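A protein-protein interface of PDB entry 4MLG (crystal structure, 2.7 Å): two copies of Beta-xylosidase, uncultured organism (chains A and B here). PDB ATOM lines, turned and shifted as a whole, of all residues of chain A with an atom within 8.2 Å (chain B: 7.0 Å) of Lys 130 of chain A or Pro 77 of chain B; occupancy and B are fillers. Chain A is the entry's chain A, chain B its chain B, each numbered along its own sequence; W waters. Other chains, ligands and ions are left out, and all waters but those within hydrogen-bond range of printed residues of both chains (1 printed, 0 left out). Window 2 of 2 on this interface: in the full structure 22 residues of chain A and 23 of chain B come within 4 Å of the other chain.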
ATOM      1  N   ARG A 109      10.074  -0.674  -5.471  1.00  0.00           N
ATOM      2  CA  ARG A 109      10.483  -1.836  -4.698  1.00  0.00           C
ATOM      3  C   ARG A 109      10.910  -1.362  -3.318  1.00  0.00           C
ATOM      4  O   ARG A 109      10.990  -0.158  -3.067  1.00  0.00           O
ATOM      5  CB  ARG A 109      11.644  -2.562  -5.380  1.00  0.00           C
ATOM      6  CG  ARG A 109      11.357  -3.040  -6.797  1.00  0.00           C
ATOM      7  CD  ARG A 109      10.263  -4.095  -6.824  1.00  0.00           C
ATOM      8  NE  ARG A 109      10.190  -4.774  -8.115  1.00  0.00           N
ATOM      9  CZ  ARG A 109       9.336  -5.752  -8.397  1.00  0.00           C
ATOM     10  NH1 ARG A 109       8.473  -6.169  -7.480  1.00  0.00           N
ATOM     11  NH2 ARG A 109       9.341  -6.315  -9.598  1.00  0.00           N
ATOM     12  N   ILE A 110      11.180  -2.307  -2.425  1.00  0.00           N
ATOM     13  CA  ILE A 110      11.626  -1.971  -1.079  1.00  0.00           C
ATOM     14  C   ILE A 110      12.961  -2.639  -0.774  1.00  0.00           C
ATOM     15  O   ILE A 110      13.090  -3.859  -0.871  1.00  0.00           O
ATOM     16  CB  ILE A 110      10.584  -2.376  -0.022  1.00  0.00           C
ATOM     17  CG1 ILE A 110       9.285  -1.595  -0.235  1.00  0.00           C
ATOM     18  CG2 ILE A 110      11.122  -2.137   1.383  1.00  0.00           C
ATOM     19  CD1 ILE A 110       8.182  -1.951   0.740  1.00  0.00           C
ATOM     20  N   GLY A 111      13.954  -1.833  -0.410  1.00  0.00           N
ATOM     21  CA  GLY A 111      15.285  -2.343  -0.142  1.00  0.00           C
ATOM     22  C   GLY A 111      15.647  -2.299   1.329  1.00  0.00           C
ATOM     23  O   GLY A 111      14.959  -1.657   2.127  1.00  0.00           O
ATOM     24  N   VAL A 112      16.731  -2.981   1.687  1.00  0.00           N
ATOM     25  CA  VAL A 112      17.181  -3.040   3.072  1.00  0.00           C
ATOM     26  C   VAL A 112      18.586  -2.466   3.237  1.00  0.00           C
ATOM     27  O   VAL A 112      19.503  -2.817   2.493  1.00  0.00           O
ATOM     28  CB  VAL A 112      17.162  -4.485   3.606  1.00  0.00           C
ATOM     29  CG1 VAL A 112      17.704  -4.539   5.027  1.00  0.00           C
ATOM     30  CG2 VAL A 112      15.754  -5.053   3.549  1.00  0.00           C
ATOM     31  N   ASN A 127      20.251  -5.854  -3.828  1.00  0.00           N
ATOM     32  CA  ASN A 127      18.976  -6.065  -4.503  1.00  0.00           C
ATOM     33  C   ASN A 127      17.790  -5.807  -3.581  1.00  0.00           C
ATOM     34  O   ASN A 127      17.899  -5.967  -2.365  1.00  0.00           O
ATOM     35  CB  ASN A 127      18.901  -7.482  -5.080  1.00  0.00           C
ATOM     36  CG  ASN A 127      19.912  -7.716  -6.186  1.00  0.00           C
ATOM     37  OD1 ASN A 127      21.007  -8.221  -5.943  1.00  0.00           O
ATOM     38  ND2 ASN A 127      19.548  -7.347  -7.410  1.00  0.00           N
ATOM     39  N   PRO A 128      16.650  -5.394  -4.155  1.00  0.00           N
ATOM     40  CA  PRO A 128      15.459  -5.153  -3.338  1.00  0.00           C
ATOM     41  C   PRO A 128      14.887  -6.455  -2.790  1.00  0.00           C
ATOM     42  O   PRO A 128      15.231  -7.529  -3.282  1.00  0.00           O
ATOM     43  CB  PRO A 128      14.479  -4.528  -4.334  1.00  0.00           C
ATOM     44  CG  PRO A 128      14.914  -5.043  -5.661  1.00  0.00           C
ATOM     45  CD  PRO A 128      16.409  -5.103  -5.579  1.00  0.00           C
ATOM     46  N   ILE A 129      14.028  -6.348  -1.782  1.00  0.00           N
ATOM     47  CA  ILE A 129      13.374  -7.509  -1.188  1.00  0.00           C
ATOM     48  C   ILE A 129      12.543  -8.259  -2.226  1.00  0.00           C
ATOM     49  O   ILE A 129      11.783  -7.654  -2.980  1.00  0.00           O
ATOM     50  CB  ILE A 129      12.462  -7.091  -0.017  1.00  0.00           C
ATOM     51  CG1 ILE A 129      13.277  -6.396   1.076  1.00  0.00           C
ATOM     52  CG2 ILE A 129      11.724  -8.294   0.553  1.00  0.00           C
ATOM     53  CD1 ILE A 129      12.444  -5.938   2.259  1.00  0.00           C
ATOM     54  N   LYS A 130      12.700  -9.578  -2.265  1.00  0.00           N
ATOM     55  CA  LYS A 130      11.969 -10.414  -3.208  1.00  0.00           C
ATOM     56  C   LYS A 130      10.462 -10.321  -2.988  1.00  0.00           C
ATOM     57  O   LYS A 130       9.974 -10.541  -1.878  1.00  0.00           O
ATOM     58  CB  LYS A 130      12.423 -11.870  -3.089  1.00  0.00           C
ATOM     59  CG  LYS A 130      13.905 -12.078  -3.349  1.00  0.00           C
ATOM     60  CD  LYS A 130      14.326 -13.499  -3.021  1.00  0.00           C
ATOM     61  CE  LYS A 130      15.775 -13.741  -3.404  1.00  0.00           C
ATOM     62  NZ  LYS A 130      16.701 -12.781  -2.742  1.00  0.00           N
ATOM     63  N   GLY A 131       9.733  -9.990  -4.048  1.00  0.00           N
ATOM     64  CA  GLY A 131       8.285  -9.914  -3.986  1.00  0.00           C
ATOM     65  C   GLY A 131       7.769  -8.560  -3.541  1.00  0.00           C
ATOM     66  O   GLY A 131       6.568  -8.297  -3.597  1.00  0.00           O
ATOM     67  N   SER A 132       8.680  -7.699  -3.100  1.00  0.00           N
ATOM     68  CA  SER A 132       8.308  -6.381  -2.594  1.00  0.00           C
ATOM     69  C   SER A 132       7.747  -5.486  -3.693  1.00  0.00           C
ATOM     70  O   SER A 132       8.156  -5.576  -4.852  1.00  0.00           O
ATOM     71  CB  SER A 132       9.509  -5.702  -1.935  1.00  0.00           C
ATOM     72  OG  SER A 132      10.559  -5.517  -2.868  1.00  0.00           O
ATOM     73  N   TYR A 133       6.808  -4.624  -3.320  1.00  0.00           N
ATOM     74  CA  TYR A 133       6.215  -3.677  -4.255  1.00  0.00           C
ATOM     75  C   TYR A 133       5.612  -2.493  -3.509  1.00  0.00           C
ATOM     76  O   TYR A 133       5.547  -2.498  -2.279  1.00  0.00           O
ATOM     77  CB  TYR A 133       5.165  -4.364  -5.134  1.00  0.00           C
ATOM     78  CG  TYR A 133       3.964  -4.910  -4.390  1.00  0.00           C
ATOM     79  CD1 TYR A 133       2.788  -4.176  -4.301  1.00  0.00           C
ATOM     80  CD2 TYR A 133       3.997  -6.165  -3.793  1.00  0.00           C
ATOM     81  CE1 TYR A 133       1.685  -4.669  -3.634  1.00  0.00           C
ATOM     82  CE2 TYR A 133       2.896  -6.667  -3.122  1.00  0.00           C
ATOM     83  CZ  TYR A 133       1.742  -5.913  -3.046  1.00  0.00           C
ATOM     84  OH  TYR A 133       0.640  -6.402  -2.382  1.00  0.00           O
ATOM     85  N   VAL A 186       2.855  -7.968   5.987  1.00  0.00           N
ATOM     86  CA  VAL A 186       3.658  -9.162   5.763  1.00  0.00           C
ATOM     87  C   VAL A 186       4.654  -9.372   6.903  1.00  0.00           C
ATOM     88  O   VAL A 186       5.245  -8.417   7.410  1.00  0.00           O
ATOM     89  CB  VAL A 186       4.383  -9.114   4.392  1.00  0.00           C
ATOM     90  CG1 VAL A 186       5.328  -7.923   4.318  1.00  0.00           C
ATOM     91  CG2 VAL A 186       5.125 -10.417   4.125  1.00  0.00           C
ATOM     92  N   ARG A 189      11.076 -12.509   8.029  1.00  0.00           N
ATOM     93  CA  ARG A 189      11.837 -13.592   8.640  1.00  0.00           C
ATOM     94  C   ARG A 189      12.942 -13.008   9.520  1.00  0.00           C
ATOM     95  O   ARG A 189      13.194 -11.804   9.486  1.00  0.00           O
ATOM     96  CB  ARG A 189      12.403 -14.541   7.581  1.00  0.00           C
ATOM     97  CG  ARG A 189      13.304 -13.883   6.556  1.00  0.00           C
ATOM     98  CD  ARG A 189      13.830 -14.899   5.550  1.00  0.00           C
ATOM     99  NE  ARG A 189      15.060 -14.445   4.908  1.00  0.00           N
ATOM    100  CZ  ARG A 189      15.594 -15.003   3.826  1.00  0.00           C
ATOM    101  NH1 ARG A 189      15.000 -16.038   3.247  1.00  0.00           N
ATOM    102  NH2 ARG A 189      16.718 -14.519   3.316  1.00  0.00           N
ATOM    103  N   LEU A 193      15.883  -9.744   5.986  1.00  0.00           N
ATOM    104  CA  LEU A 193      16.290  -9.425   4.622  1.00  0.00           C
ATOM    105  C   LEU A 193      15.196  -9.751   3.610  1.00  0.00           C
ATOM    106  O   LEU A 193      15.151  -9.172   2.524  1.00  0.00           O
ATOM    107  CB  LEU A 193      17.575 -10.169   4.257  1.00  0.00           C
ATOM    108  CG  LEU A 193      18.794  -9.895   5.137  1.00  0.00           C
ATOM    109  CD1 LEU A 193      20.014 -10.636   4.611  1.00  0.00           C
ATOM    110  CD2 LEU A 193      19.067  -8.401   5.232  1.00  0.00           C
ATOM    111  N   GLU A 194      14.320 -10.687   3.965  1.00  0.00           N
ATOM    112  CA  GLU A 194      13.250 -11.107   3.067  1.00  0.00           C
ATOM    113  C   GLU A 194      11.933 -11.298   3.807  1.00  0.00           C
ATOM    114  O   GLU A 194      11.896 -11.298   5.038  1.00  0.00           O
ATOM    115  CB  GLU A 194      13.623 -12.410   2.350  1.00  0.00           C
ATOM    116  CG  GLU A 194      14.840 -12.313   1.443  1.00  0.00           C
ATOM    117  CD  GLU A 194      14.613 -11.419   0.238  1.00  0.00           C
ATOM    118  OE1 GLU A 194      13.441 -11.128  -0.083  1.00  0.00           O
ATOM    119  OE2 GLU A 194      15.610 -11.007  -0.392  1.00  0.00           O
ATOM    120  N   PHE A 195      10.855 -11.459   3.045  1.00  0.00           N
ATOM    121  CA  PHE A 195       9.548 -11.761   3.614  1.00  0.00           C
ATOM    122  C   PHE A 195       9.526 -13.210   4.087  1.00  0.00           C
ATOM    123  O   PHE A 195      10.175 -14.070   3.494  1.00  0.00           O
ATOM    124  CB  PHE A 195       8.441 -11.536   2.579  1.00  0.00           C
ATOM    125  CG  PHE A 195       8.283 -10.103   2.151  1.00  0.00           C
ATOM    126  CD1 PHE A 195       8.781  -9.066   2.929  1.00  0.00           C
ATOM    127  CD2 PHE A 195       7.627  -9.791   0.970  1.00  0.00           C
ATOM    128  CE1 PHE A 195       8.633  -7.743   2.531  1.00  0.00           C
ATOM    129  CE2 PHE A 195       7.474  -8.473   0.568  1.00  0.00           C
ATOM    130  CZ  PHE A 195       7.978  -7.448   1.349  1.00  0.00           C
ATOM    131  N   ALA A 196       8.787 -13.478   5.156  1.00  0.00           N
ATOM    132  CA  ALA A 196       8.658 -14.840   5.667  1.00  0.00           C
ATOM    133  C   ALA A 196       7.433 -15.520   5.065  1.00  0.00           C
ATOM    134  O   ALA A 196       7.303 -16.743   5.106  1.00  0.00           O
ATOM    135  CB  ALA A 196       8.570 -14.834   7.185  1.00  0.00           C
ATOM    136  N   GLU A 197       6.540 -14.712   4.506  1.00  0.00           N
ATOM    137  CA  GLU A 197       5.294 -15.209   3.940  1.00  0.00           C
ATOM    138  C   GLU A 197       4.823 -14.278   2.832  1.00  0.00           C
ATOM    139  O   GLU A 197       5.507 -13.313   2.490  1.00  0.00           O
ATOM    140  CB  GLU A 197       4.217 -15.285   5.023  1.00  0.00           C
ATOM    141  CG  GLU A 197       3.870 -13.929   5.619  1.00  0.00           C
ATOM    142  CD  GLU A 197       2.756 -14.001   6.641  1.00  0.00           C
ATOM    143  OE1 GLU A 197       2.292 -15.121   6.936  1.00  0.00           O
ATOM    144  OE2 GLU A 197       2.344 -12.934   7.145  1.00  0.00           O
ATOM    145  N   PRO A 199       2.451 -11.334   1.499  1.00  0.00           N
ATOM    146  CA  PRO A 199       1.692 -10.189   2.013  1.00  0.00           C
ATOM    147  C   PRO A 199       0.193 -10.381   1.809  1.00  0.00           C
ATOM    148  O   PRO A 199      -0.218 -11.106   0.903  1.00  0.00           O
ATOM    149  CB  PRO A 199       2.194  -9.026   1.154  1.00  0.00           C
ATOM    150  CG  PRO A 199       3.557  -9.444   0.716  1.00  0.00           C
ATOM    151  CD  PRO A 199       3.468 -10.927   0.514  1.00  0.00           C
ATOM    152  N   THR B  73      12.746 -24.390 -11.015  1.00  0.00           N
ATOM    153  CA  THR B  73      12.241 -23.202 -10.328  1.00  0.00           C
ATOM    154  C   THR B  73      12.476 -23.243  -8.822  1.00  0.00           C
ATOM    155  O   THR B  73      12.768 -22.221  -8.204  1.00  0.00           O
ATOM    156  CB  THR B  73      10.731 -23.004 -10.580  1.00  0.00           C
ATOM    157  OG1 THR B  73      10.019 -24.174 -10.160  1.00  0.00           O
ATOM    158  CG2 THR B  73      10.462 -22.750 -12.056  1.00  0.00           C
ATOM    159  N   GLU B  74      12.364 -24.432  -8.242  1.00  0.00           N
ATOM    160  CA  GLU B  74      12.504 -24.609  -6.799  1.00  0.00           C
ATOM    161  C   GLU B  74      13.904 -24.271  -6.284  1.00  0.00           C
ATOM    162  O   GLU B  74      14.099 -24.091  -5.082  1.00  0.00           O
ATOM    163  CB  GLU B  74      12.131 -26.040  -6.413  1.00  0.00           C
ATOM    164  CG  GLU B  74      10.754 -26.462  -6.899  1.00  0.00           C
ATOM    165  CD  GLU B  74      10.658 -27.951  -7.153  1.00  0.00           C
ATOM    166  OE1 GLU B  74      11.672 -28.652  -6.957  1.00  0.00           O
ATOM    167  OE2 GLU B  74       9.572 -28.421  -7.552  1.00  0.00           O
ATOM    168  N   ASP B  75      14.873 -24.183  -7.189  1.00  0.00           N
ATOM    169  CA  ASP B  75      16.246 -23.869  -6.804  1.00  0.00           C
ATOM    170  C   ASP B  75      16.527 -22.368  -6.854  1.00  0.00           C
ATOM    171  O   ASP B  75      17.450 -21.877  -6.205  1.00  0.00           O
ATOM    172  CB  ASP B  75      17.245 -24.621  -7.687  1.00  0.00           C
ATOM    173  CG  ASP B  75      17.131 -26.126  -7.544  1.00  0.00           C
ATOM    174  OD1 ASP B  75      16.624 -26.591  -6.501  1.00  0.00           O
ATOM    175  OD2 ASP B  75      17.552 -26.843  -8.475  1.00  0.00           O
ATOM    176  N   ILE B  76      15.724 -21.644  -7.624  1.00  0.00           N
ATOM    177  CA  ILE B  76      15.896 -20.205  -7.778  1.00  0.00           C
ATOM    178  C   ILE B  76      15.366 -19.457  -6.555  1.00  0.00           C
ATOM    179  O   ILE B  76      14.194 -19.577  -6.213  1.00  0.00           O
ATOM    180  CB  ILE B  76      15.189 -19.704  -9.049  1.00  0.00           C
ATOM    181  CG1 ILE B  76      15.604 -20.563 -10.248  1.00  0.00           C
ATOM    182  CG2 ILE B  76      15.502 -18.237  -9.294  1.00  0.00           C
ATOM    183  CD1 ILE B  76      14.772 -20.340 -11.491  1.00  0.00           C
ATOM    184  N   PRO B  77      16.240 -18.694  -5.881  1.00  0.00           N
ATOM    185  CA  PRO B  77      15.875 -17.978  -4.652  1.00  0.00           C
ATOM    186  C   PRO B  77      14.771 -16.936  -4.843  1.00  0.00           C
ATOM    187  O   PRO B  77      14.000 -16.694  -3.914  1.00  0.00           O
ATOM    188  CB  PRO B  77      17.185 -17.295  -4.248  1.00  0.00           C
ATOM    189  CG  PRO B  77      18.247 -18.155  -4.846  1.00  0.00           C
ATOM    190  CD  PRO B  77      17.682 -18.597  -6.163  1.00  0.00           C
ATOM    191  N   TRP B  78      14.698 -16.330  -6.023  1.00  0.00           N
ATOM    192  CA  TRP B  78      13.684 -15.316  -6.294  1.00  0.00           C
ATOM    193  C   TRP B  78      12.527 -15.882  -7.105  1.00  0.00           C
ATOM    194  O   TRP B  78      11.773 -15.136  -7.728  1.00  0.00           O
ATOM    195  CB  TRP B  78      14.292 -14.109  -7.018  1.00  0.00           C
ATOM    196  CG  TRP B  78      14.982 -14.428  -8.324  1.00  0.00           C
ATOM    197  CD1 TRP B  78      16.273 -14.843  -8.487  1.00  0.00           C
ATOM    198  CD2 TRP B  78      14.425 -14.332  -9.645  1.00  0.00           C
ATOM    199  NE1 TRP B  78      16.551 -15.019  -9.820  1.00  0.00           N
ATOM    200  CE2 TRP B  78      15.435 -14.713 -10.552  1.00  0.00           C
ATOM    201  CE3 TRP B  78      13.172 -13.965 -10.147  1.00  0.00           C
ATOM    202  CZ2 TRP B  78      15.228 -14.739 -11.932  1.00  0.00           C
ATOM    203  CZ3 TRP B  78      12.970 -13.992 -11.516  1.00  0.00           C
ATOM    204  CH2 TRP B  78      13.993 -14.377 -12.392  1.00  0.00           C
ATOM    205  N   ALA B  79      12.384 -17.202  -7.074  1.00  0.00           N
ATOM    206  CA  ALA B  79      11.428 -17.891  -7.933  1.00  0.00           C
ATOM    207  C   ALA B  79       9.981 -17.462  -7.743  1.00  0.00           C
ATOM    208  O   ALA B  79       9.493 -17.318  -6.622  1.00  0.00           O
ATOM    209  CB  ALA B  79      11.544 -19.390  -7.764  1.00  0.00           C
ATOM    210  N   GLY B  80       9.308 -17.258  -8.868  1.00  0.00           N
ATOM    211  CA  GLY B  80       7.871 -17.099  -8.893  1.00  0.00           C
ATOM    212  C   GLY B  80       7.289 -18.295  -9.616  1.00  0.00           C
ATOM    213  O   GLY B  80       6.938 -19.291  -8.989  1.00  0.00           O
ATOM    214  N   PHE B  99      17.889 -17.038 -18.082  1.00  0.00           N
ATOM    215  CA  PHE B  99      16.536 -17.575 -18.069  1.00  0.00           C
ATOM    216  C   PHE B  99      15.506 -16.521 -17.680  1.00  0.00           C
ATOM    217  O   PHE B  99      15.758 -15.692 -16.805  1.00  0.00           O
ATOM    218  CB  PHE B  99      16.447 -18.765 -17.107  1.00  0.00           C
ATOM    219  CG  PHE B  99      16.792 -18.423 -15.681  1.00  0.00           C
ATOM    220  CD1 PHE B  99      15.800 -18.081 -14.776  1.00  0.00           C
ATOM    221  CD2 PHE B  99      18.107 -18.449 -15.246  1.00  0.00           C
ATOM    222  CE1 PHE B  99      16.114 -17.766 -13.467  1.00  0.00           C
ATOM    223  CE2 PHE B  99      18.427 -18.136 -13.937  1.00  0.00           C
ATOM    224  CZ  PHE B  99      17.428 -17.795 -13.046  1.00  0.00           C
ATOM    225  N   ASP B 103       8.764 -12.984 -11.383  1.00  0.00           N
ATOM    226  CA  ASP B 103       9.138 -12.871  -9.978  1.00  0.00           C
ATOM    227  C   ASP B 103       7.954 -13.191  -9.070  1.00  0.00           C
ATOM    228  O   ASP B 103       6.917 -13.669  -9.530  1.00  0.00           O
ATOM    229  CB  ASP B 103       9.708 -11.483  -9.662  1.00  0.00           C
ATOM    230  CG  ASP B 103       8.792 -10.350 -10.101  1.00  0.00           C
ATOM    231  OD1 ASP B 103       7.567 -10.565 -10.217  1.00  0.00           O
ATOM    232  OD2 ASP B 103       9.304  -9.233 -10.324  1.00  0.00           O
ATOM    233  N   GLN B 104       8.100 -12.910  -7.780  1.00  0.00           N
ATOM    234  CA  GLN B 104       7.028 -13.181  -6.829  1.00  0.00           C
ATOM    235  C   GLN B 104       5.866 -12.201  -6.989  1.00  0.00           C
ATOM    236  O   GLN B 104       4.886 -12.261  -6.247  1.00  0.00           O
ATOM    237  CB  GLN B 104       7.569 -13.173  -5.399  1.00  0.00           C
ATOM    238  CG  GLN B 104       8.650 -14.216  -5.166  1.00  0.00           C
ATOM    239  CD  GLN B 104       9.214 -14.186  -3.760  1.00  0.00           C
ATOM    240  OE1 GLN B 104       8.768 -13.413  -2.913  1.00  0.00           O
ATOM    241  NE2 GLN B 104      10.206 -15.033  -3.507  1.00  0.00           N
ATOM    242  N   ASN B 105       5.984 -11.307  -7.968  1.00  0.00           N
ATOM    243  CA  ASN B 105       4.919 -10.369  -8.297  1.00  0.00           C
ATOM    244  C   ASN B 105       4.362 -10.620  -9.697  1.00  0.00           C
ATOM    245  O   ASN B 105       3.650  -9.777 -10.250  1.00  0.00           O
ATOM    246  CB  ASN B 105       5.427  -8.932  -8.186  1.00  0.00           C
ATOM    247  CG  ASN B 105       5.968  -8.611  -6.808  1.00  0.00           C
ATOM    248  OD1 ASN B 105       7.168  -8.400  -6.633  1.00  0.00           O
ATOM    249  ND2 ASN B 105       5.082  -8.567  -5.819  1.00  0.00           N
ATOM    250  N   PRO B 124      21.849 -20.964 -10.054  1.00  0.00           N
ATOM    251  CA  PRO B 124      21.251 -19.648 -10.300  1.00  0.00           C
ATOM    252  C   PRO B 124      21.672 -18.598  -9.277  1.00  0.00           C
ATOM    253  O   PRO B 124      21.936 -18.926  -8.120  1.00  0.00           O
ATOM    254  CB  PRO B 124      19.753 -19.929 -10.173  1.00  0.00           C
ATOM    255  CG  PRO B 124      19.675 -21.050  -9.198  1.00  0.00           C
ATOM    256  CD  PRO B 124      20.889 -21.904  -9.449  1.00  0.00           C
ATOM    257  N   GLN B 125      21.736 -17.344  -9.713  1.00  0.00           N
ATOM    258  CA  GLN B 125      22.000 -16.227  -8.816  1.00  0.00           C
ATOM    259  C   GLN B 125      20.777 -15.984  -7.941  1.00  0.00           C
ATOM    260  O   GLN B 125      19.660 -16.346  -8.311  1.00  0.00           O
ATOM    261  CB  GLN B 125      22.340 -14.969  -9.615  1.00  0.00           C
ATOM    262  CG  GLN B 125      23.686 -15.023 -10.323  1.00  0.00           C
ATOM    263  CD  GLN B 125      24.854 -14.928  -9.359  1.00  0.00           C
ATOM    264  OE1 GLN B 125      25.036 -13.915  -8.683  1.00  0.00           O
ATOM    265  NE2 GLN B 125      25.651 -15.989  -9.287  1.00  0.00           N
ATOM    266  N   GLU B 126      20.987 -15.366  -6.783  1.00  0.00           N
ATOM    267  CA  GLU B 126      19.905 -15.166  -5.823  1.00  0.00           C
ATOM    268  C   GLU B 126      18.863 -14.149  -6.281  1.00  0.00           C
ATOM    269  O   GLU B 126      17.702 -14.224  -5.888  1.00  0.00           O
ATOM    270  CB  GLU B 126      20.460 -14.775  -4.451  1.00  0.00           C
ATOM    271  CG  GLU B 126      21.291 -15.859  -3.790  1.00  0.00           C
ATOM    272  CD  GLU B 126      21.547 -15.584  -2.322  1.00  0.00           C
ATOM    273  OE1 GLU B 126      20.910 -14.661  -1.769  1.00  0.00           O
ATOM    274  OE2 GLU B 126      22.381 -16.291  -1.720  1.00  0.00           O
ATOM    275  N   ASN B 127      19.281 -13.203  -7.113  1.00  0.00           N
ATOM    276  CA  ASN B 127      18.383 -12.163  -7.600  1.00  0.00           C
ATOM    277  C   ASN B 127      18.463 -12.009  -9.114  1.00  0.00           C
ATOM    278  O   ASN B 127      19.505 -12.282  -9.711  1.00  0.00           O
ATOM    279  CB  ASN B 127      18.701 -10.834  -6.915  1.00  0.00           C
ATOM    280  CG  ASN B 127      18.505 -10.892  -5.415  1.00  0.00           C
ATOM    281  OD1 ASN B 127      17.404 -10.665  -4.915  1.00  0.00           O
ATOM    282  ND2 ASN B 127      19.574 -11.197  -4.688  1.00  0.00           N
ATOM    283  N   PRO B 128      17.362 -11.570  -9.744  1.00  0.00           N
ATOM    284  CA  PRO B 128      17.363 -11.367 -11.196  1.00  0.00           C
ATOM    285  C   PRO B 128      18.245 -10.188 -11.594  1.00  0.00           C
ATOM    286  O   PRO B 128      18.665  -9.416 -10.731  1.00  0.00           O
ATOM    287  CB  PRO B 128      15.898 -11.050 -11.503  1.00  0.00           C
ATOM    288  CG  PRO B 128      15.365 -10.477 -10.238  1.00  0.00           C
ATOM    289  CD  PRO B 128      16.059 -11.228  -9.141  1.00  0.00           C
HETATM  290  O   HOH W   1      15.089  -9.359  -5.449  1.00  0.00           O
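Asn 127 of chain B touches its own counterpart, Asn 127 of chain A.
Positions printed for both chains: 127 and 128.
Of the 12 pairs that touch across the chains among the printed residues, 1 has its exchanged pair printed and touching as well.
Hydrophobic or aromatic side chains of chain A within 4 Å of the printed part of chain B: Tyr 133.
Hydrophobic or aromatic side chains of chain B that line the printed part of chain A: Pro 77 and Trp 78.
Among the printed residues, 12 pairs touch across the chains.
Among the printed residues, Asp or Glu carboxylates within 4 Å of a Lys or Arg side-chain nitrogen of the other chain: Arg 109 of chain A with Asp 103 of chain B (3.0 Å).
Water W1 lies within hydrogen-bond range of OD1 of Asn 127 of chain B (2.7 Å) and O of Pro 128 of chain A (2.8 Å).
The guanidinium group (NH1) of Arg 109 of chain A sits at hydrogen-bond distance from the backbone carbonyl oxygen (O) of Ser 132 of chain A, at 2.7 Å.
The backbone NH (N) of Ile 110 of chain A lies within hydrogen-bond range of the side-chain hydroxyl (OG) of Ser 132 of chain A, at 3.3 Å.
The backbone carbonyl oxygen (O) of Ile 129 of chain A lies within hydrogen-bond range of the side-chain hydroxyl (OG) of Ser 132 of chain A (2.5 Å).
The side-chain amino group (NZ) of Lys 130 of chain A is in salt-bridge range of the side-chain carboxylate (OE2) of Glu 194 of chain A (3.1 Å).
OD1 of Asp 103 of chain B sits at hydrogen-bond distance from N of Asn 105 of chain B, 2.8 Å away.
Asn 127 of chain B touches Asn 127 of chain A (CB to CG, 3.4 Å).
O of Pro 77 of chain B touches CD of Lys 130 of chain A, 3.3 Å away.
CD of Lys 130 of chain A touches CA of Trp 78 of chain B, 3.8 Å away.
O of Glu 126 of chain B touches CE of Lys 130 of chain A, at 3.2 Å.
Gly 131 of chain A touches Gln 104 of chain B (CA to CB, 3.6 Å).
Tyr 133 of chain A touches Asn 105 of chain B.
Lys 130 of chain A touches five residues of chain B.
Of chain A, only Lys 130 (3.3 Å) comes within 4 Å of Pro 77 of chain B.
Of the printed residues of chain A, Gln 104 of chain B touches Lys 130 and Gly 131.
Printed residues of chain B within 4 Å of Ser 132 of chain A: Asn 105.
Ile 76 of chain B touches none of the printed residues of chain A.
Pro 128 of chain B touches none of the printed residues of chain A.
The nearest residue of chain A that does not touch Pro 77 of chain B is Glu 194 of chain A (6.7 Å).
NH2 of Arg 109 of chain A is in salt-bridge range of OD2 of Asp 103 of chain B, at 3.0 Å.
The guanidinium group (NH1) of Arg 109 of chain A sits at hydrogen-bond distance from the side-chain amide oxygen (OD1) of Asn 105 of chain B, 2.7 Å away.
The backbone carbonyl oxygen of Lys 130 of chain A sits close to the side-chain amide oxygen of Gln 104 of chain B, 3.3 Å away.
The side-chain amino group (NZ) of Lys 130 of chain A lies within hydrogen-bond range of the side-chain amide oxygen (OD1) of Asn 127 of chain B, at 3.1 Å.
ND2 of Asn 105 of chain B is in hydrogen-bond range of O of Gly 131 of chain A.
The backbone carbonyl oxygen (O) of Ser 132 of chain A lies close to the side-chain amide oxygen (OD1) of Asn 105 of chain B, 3.5 Å away.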
